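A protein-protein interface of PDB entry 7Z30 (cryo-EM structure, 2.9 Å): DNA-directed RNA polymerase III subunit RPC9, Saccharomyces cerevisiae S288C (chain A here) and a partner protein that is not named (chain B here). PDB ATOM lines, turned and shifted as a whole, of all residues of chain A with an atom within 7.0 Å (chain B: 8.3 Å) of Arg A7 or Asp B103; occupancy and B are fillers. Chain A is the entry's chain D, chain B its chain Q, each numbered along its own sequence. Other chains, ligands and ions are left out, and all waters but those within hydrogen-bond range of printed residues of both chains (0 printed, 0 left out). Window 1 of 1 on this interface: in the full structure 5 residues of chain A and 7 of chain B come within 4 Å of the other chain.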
ATOM      1  N   VAL A   3       3.250 -32.952  -3.204  1.00  0.00           N
ATOM      2  CA  VAL A   3       1.915 -32.382  -3.343  1.00  0.00           C
ATOM      3  C   VAL A   3       1.993 -31.184  -4.279  1.00  0.00           C
ATOM      4  O   VAL A   3       2.727 -30.224  -4.016  1.00  0.00           O
ATOM      5  CB  VAL A   3       1.350 -31.986  -1.971  1.00  0.00           C
ATOM      6  CG1 VAL A   3       0.229 -30.973  -2.131  1.00  0.00           C
ATOM      7  CG2 VAL A   3       0.860 -33.216  -1.225  1.00  0.00           C
ATOM      8  N   GLU A   5      -0.239 -28.762  -5.258  1.00  0.00           N
ATOM      9  CA  GLU A   5      -0.677 -27.513  -4.641  1.00  0.00           C
ATOM     10  C   GLU A   5      -1.701 -27.816  -3.556  1.00  0.00           C
ATOM     11  O   GLU A   5      -2.525 -28.723  -3.703  1.00  0.00           O
ATOM     12  CB  GLU A   5      -1.222 -26.521  -5.688  1.00  0.00           C
ATOM     13  CG  GLU A   5      -2.698 -26.614  -6.042  1.00  0.00           C
ATOM     14  CD  GLU A   5      -3.132 -28.023  -6.378  1.00  0.00           C
ATOM     15  OE1 GLU A   5      -2.368 -28.736  -7.060  1.00  0.00           O
ATOM     16  OE2 GLU A   5      -4.230 -28.421  -5.944  1.00  0.00           O
ATOM     17  N   GLU A   6      -1.610 -27.084  -2.447  1.00  0.00           N
ATOM     18  CA  GLU A   6      -2.430 -27.395  -1.283  1.00  0.00           C
ATOM     19  C   GLU A   6      -3.895 -27.054  -1.526  1.00  0.00           C
ATOM     20  O   GLU A   6      -4.786 -27.864  -1.238  1.00  0.00           O
ATOM     21  CB  GLU A   6      -1.906 -26.639  -0.062  1.00  0.00           C
ATOM     22  CG  GLU A   6      -1.095 -27.486   0.904  1.00  0.00           C
ATOM     23  CD  GLU A   6       0.281 -27.835   0.363  1.00  0.00           C
ATOM     24  OE1 GLU A   6       0.968 -26.926  -0.149  1.00  0.00           O
ATOM     25  OE2 GLU A   6       0.676 -29.016   0.446  1.00  0.00           O
ATOM     26  N   ARG A   7      -4.162 -25.862  -2.047  1.00  0.00           N
ATOM     27  CA  ARG A   7      -5.507 -25.300  -2.137  1.00  0.00           C
ATOM     28  C   ARG A   7      -6.082 -25.594  -3.521  1.00  0.00           C
ATOM     29  O   ARG A   7      -5.974 -24.778  -4.438  1.00  0.00           O
ATOM     30  CB  ARG A   7      -5.468 -23.800  -1.862  1.00  0.00           C
ATOM     31  CG  ARG A   7      -6.722 -23.233  -1.227  1.00  0.00           C
ATOM     32  CD  ARG A   7      -6.468 -21.816  -0.742  1.00  0.00           C
ATOM     33  NE  ARG A   7      -5.484 -21.785   0.334  1.00  0.00           N
ATOM     34  CZ  ARG A   7      -4.219 -21.414   0.180  1.00  0.00           C
ATOM     35  NH1 ARG A   7      -3.753 -21.018  -0.994  1.00  0.00           N
ATOM     36  NH2 ARG A   7      -3.403 -21.437   1.231  1.00  0.00           N
ATOM     37  N   ASN A   8      -6.700 -26.761  -3.667  1.00  0.00           N
ATOM     38  CA  ASN A   8      -7.392 -27.097  -4.900  1.00  0.00           C
ATOM     39  C   ASN A   8      -8.819 -26.553  -4.824  1.00  0.00           C
ATOM     40  O   ASN A   8      -9.159 -25.775  -3.928  1.00  0.00           O
ATOM     41  CB  ASN A   8      -7.353 -28.605  -5.146  1.00  0.00           C
ATOM     42  CG  ASN A   8      -7.517 -28.963  -6.614  1.00  0.00           C
ATOM     43  OD1 ASN A   8      -6.602 -28.776  -7.417  1.00  0.00           O
ATOM     44  ND2 ASN A   8      -8.685 -29.486  -6.970  1.00  0.00           N
ATOM     45  N   ALA A   9      -9.666 -26.950  -5.772  1.00  0.00           N
ATOM     46  CA  ALA A   9     -11.038 -26.460  -5.810  1.00  0.00           C
ATOM     47  C   ALA A   9     -11.775 -26.802  -4.519  1.00  0.00           C
ATOM     48  O   ALA A   9     -11.578 -27.872  -3.935  1.00  0.00           O
ATOM     49  CB  ALA A   9     -11.777 -27.049  -7.013  1.00  0.00           C
ATOM     50  N   PHE A  10     -12.622 -25.877  -4.074  1.00  0.00           N
ATOM     51  CA  PHE A  10     -13.391 -26.066  -2.855  1.00  0.00           C
ATOM     52  C   PHE A  10     -14.456 -27.143  -3.045  1.00  0.00           C
ATOM     53  O   PHE A  10     -14.804 -27.530  -4.164  1.00  0.00           O
ATOM     54  CB  PHE A  10     -14.046 -24.754  -2.426  1.00  0.00           C
ATOM     55  CG  PHE A  10     -13.095 -23.785  -1.797  1.00  0.00           C
ATOM     56  CD1 PHE A  10     -12.782 -23.887  -0.453  1.00  0.00           C
ATOM     57  CD2 PHE A  10     -12.506 -22.781  -2.546  1.00  0.00           C
ATOM     58  CE1 PHE A  10     -11.907 -23.001   0.138  1.00  0.00           C
ATOM     59  CE2 PHE A  10     -11.627 -21.891  -1.960  1.00  0.00           C
ATOM     60  CZ  PHE A  10     -11.328 -22.004  -0.615  1.00  0.00           C
ATOM     61  N   LYS A 117     -16.971 -12.792  -0.619  1.00  0.00           N
ATOM     62  CA  LYS A 117     -16.354 -13.832   0.185  1.00  0.00           C
ATOM     63  C   LYS A 117     -16.760 -15.196  -0.354  1.00  0.00           C
ATOM     64  O   LYS A 117     -17.918 -15.418  -0.720  1.00  0.00           O
ATOM     65  CB  LYS A 117     -16.747 -13.691   1.661  1.00  0.00           C
ATOM     66  CG  LYS A 117     -15.868 -14.484   2.590  1.00  0.00           C
ATOM     67  CD  LYS A 117     -14.443 -14.498   2.085  1.00  0.00           C
ATOM     68  CE  LYS A 117     -13.676 -15.632   2.708  1.00  0.00           C
ATOM     69  NZ  LYS A 117     -13.873 -16.850   1.886  1.00  0.00           N
ATOM     70  N   THR B 101      -3.436 -15.692   5.768  1.00  0.00           N
ATOM     71  CA  THR B 101      -2.279 -16.559   5.957  1.00  0.00           C
ATOM     72  C   THR B 101      -1.993 -17.381   4.706  1.00  0.00           C
ATOM     73  O   THR B 101      -2.131 -18.606   4.708  1.00  0.00           O
ATOM     74  CB  THR B 101      -2.474 -17.508   7.155  1.00  0.00           C
ATOM     75  OG1 THR B 101      -3.508 -18.455   6.855  1.00  0.00           O
ATOM     76  CG2 THR B 101      -2.850 -16.725   8.400  1.00  0.00           C
ATOM     77  N   ASN B 102      -1.604 -16.684   3.638  1.00  0.00           N
ATOM     78  CA  ASN B 102      -1.240 -17.306   2.363  1.00  0.00           C
ATOM     79  C   ASN B 102      -2.394 -18.127   1.789  1.00  0.00           C
ATOM     80  O   ASN B 102      -2.190 -19.050   0.997  1.00  0.00           O
ATOM     81  CB  ASN B 102       0.022 -18.160   2.505  1.00  0.00           C
ATOM     82  CG  ASN B 102       1.114 -17.458   3.294  1.00  0.00           C
ATOM     83  OD1 ASN B 102       1.381 -17.802   4.445  1.00  0.00           O
ATOM     84  ND2 ASN B 102       1.746 -16.464   2.679  1.00  0.00           N
ATOM     85  N   ASP B 103      -3.616 -17.787   2.182  1.00  0.00           N
ATOM     86  CA  ASP B 103      -4.811 -18.398   1.624  1.00  0.00           C
ATOM     87  C   ASP B 103      -5.189 -17.676   0.340  1.00  0.00           C
ATOM     88  O   ASP B 103      -5.148 -16.444   0.276  1.00  0.00           O
ATOM     89  CB  ASP B 103      -5.977 -18.356   2.619  1.00  0.00           C
ATOM     90  CG  ASP B 103      -6.089 -17.021   3.337  1.00  0.00           C
ATOM     91  OD1 ASP B 103      -5.216 -16.152   3.132  1.00  0.00           O
ATOM     92  OD2 ASP B 103      -7.057 -16.839   4.103  1.00  0.00           O
ATOM     93  N   GLY B 104      -5.565 -18.443  -0.682  1.00  0.00           N
ATOM     94  CA  GLY B 104      -6.044 -17.837  -1.912  1.00  0.00           C
ATOM     95  C   GLY B 104      -7.348 -17.080  -1.764  1.00  0.00           C
ATOM     96  O   GLY B 104      -7.796 -16.454  -2.729  1.00  0.00           O
ATOM     97  N   ILE B 105      -7.968 -17.146  -0.589  1.00  0.00           N
ATOM     98  CA  ILE B 105      -9.252 -16.521  -0.293  1.00  0.00           C
ATOM     99  C   ILE B 105      -9.039 -15.460   0.784  1.00  0.00           C
ATOM    100  O   ILE B 105      -8.325 -15.694   1.767  1.00  0.00           O
ATOM    101  CB  ILE B 105     -10.281 -17.599   0.098  1.00  0.00           C
ATOM    102  CG1 ILE B 105     -10.247 -17.931   1.594  1.00  0.00           C
ATOM    103  CG2 ILE B 105     -10.048 -18.841  -0.726  1.00  0.00           C
ATOM    104  CD1 ILE B 105     -11.458 -18.700   2.078  1.00  0.00           C
ATOM    105  N   GLU B 106      -9.594 -14.269   0.559  1.00  0.00           N
ATOM    106  CA  GLU B 106      -9.381 -13.113   1.426  1.00  0.00           C
ATOM    107  C   GLU B 106     -10.574 -12.967   2.364  1.00  0.00           C
ATOM    108  O   GLU B 106     -11.716 -12.851   1.910  1.00  0.00           O
ATOM    109  CB  GLU B 106      -9.174 -11.850   0.591  1.00  0.00           C
ATOM    110  CG  GLU B 106      -8.291 -10.793   1.236  1.00  0.00           C
ATOM    111  CD  GLU B 106      -6.819 -11.171   1.261  1.00  0.00           C
ATOM    112  OE1 GLU B 106      -6.344 -11.840   0.318  1.00  0.00           O
ATOM    113  OE2 GLU B 106      -6.132 -10.796   2.233  1.00  0.00           O
ATOM    114  N   ARG B 107     -10.307 -12.977   3.668  1.00  0.00           N
ATOM    115  CA  ARG B 107     -11.343 -12.714   4.656  1.00  0.00           C
ATOM    116  C   ARG B 107     -11.802 -11.264   4.573  1.00  0.00           C
ATOM    117  O   ARG B 107     -11.049 -10.376   4.167  1.00  0.00           O
ATOM    118  CB  ARG B 107     -10.826 -13.012   6.062  1.00  0.00           C
ATOM    119  CG  ARG B 107     -10.870 -14.471   6.434  1.00  0.00           C
ATOM    120  CD  ARG B 107      -9.494 -15.103   6.334  1.00  0.00           C
ATOM    121  NE  ARG B 107      -8.519 -14.507   7.239  1.00  0.00           N
ATOM    122  CZ  ARG B 107      -7.205 -14.585   7.076  1.00  0.00           C
ATOM    123  NH1 ARG B 107      -6.672 -15.229   6.051  1.00  0.00           N
ATOM    124  NH2 ARG B 107      -6.406 -14.012   7.971  1.00  0.00           N
ATOM    125  N   ASP B 110      -9.680  -8.963   6.330  1.00  0.00           N
ATOM    126  CA  ASP B 110      -8.547  -8.488   5.547  1.00  0.00           C
ATOM    127  C   ASP B 110      -8.931  -7.350   4.611  1.00  0.00           C
ATOM    128  O   ASP B 110      -8.043  -6.669   4.086  1.00  0.00           O
ATOM    129  CB  ASP B 110      -7.945  -9.643   4.744  1.00  0.00           C
ATOM    130  CG  ASP B 110      -7.250 -10.665   5.623  1.00  0.00           C
ATOM    131  OD1 ASP B 110      -7.467 -10.635   6.854  1.00  0.00           O
ATOM    132  OD2 ASP B 110      -6.492 -11.500   5.086  1.00  0.00           O
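NH1 of Arg A7 sits close to N of Gly B104.
The backbone carbonyl oxygen (O) of Asn B102 is in hydrogen-bond range of the guanidinium group (NH2) of Arg A7 (2.7 Å).
The side-chain carboxylate (OD1) of Asp B103 is in hydrogen-bond range of the backbone NH (N) of Thr B101 (3.2 Å).
The side-chain carboxylate of Asp B103 is in salt-bridge range of the guanidinium group of Arg B107 (2.6 Å).
Among the printed residues, merely in contact across the chains: Lys A117 with Ile B105 (3.0 Å), Lys A117 with Glu B106 (3.2 Å), Arg A7 with Asp B103 (3.4 Å) and Phe A10 with Ile B105 (3.4 Å).
Asp B103 touches just one residue of chain A: Arg A7 (3.4 Å).
Of the printed residues of chain B, Lys A117 touches Ile B105 and Glu B106.
Of the printed residues of chain A, Gly B104 touches Arg A7.
Of the printed residues of chain A, Ile B105 touches Phe A10 (3.4 Å) and Lys A117 (3.0 Å).
Glu A6 touches none of the printed residues of chain B.
The nearest printed residue of chain B that does not touch Arg A7 is Ile B105 (4.7 Å).
The nearest printed residue of chain A that does not touch Ile B105 is Arg A7 (4.7 Å).
Of the 8 printed residues of chain B, 5 touch a printed residue of chain A.
Hydrophobic or aromatic side chains of chain B within 4 Å of the printed part of chain A: Ile B105.
Hydrophobic or aromatic side chains of chain A that line the printed part of chain B: Phe A10.
Among the printed residues, 6 pairs touch across the chains.
Among the printed residues, no Asp or Glu carboxylate lies within 4 Å of a Lys or Arg side-chain nitrogen of the other chain.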
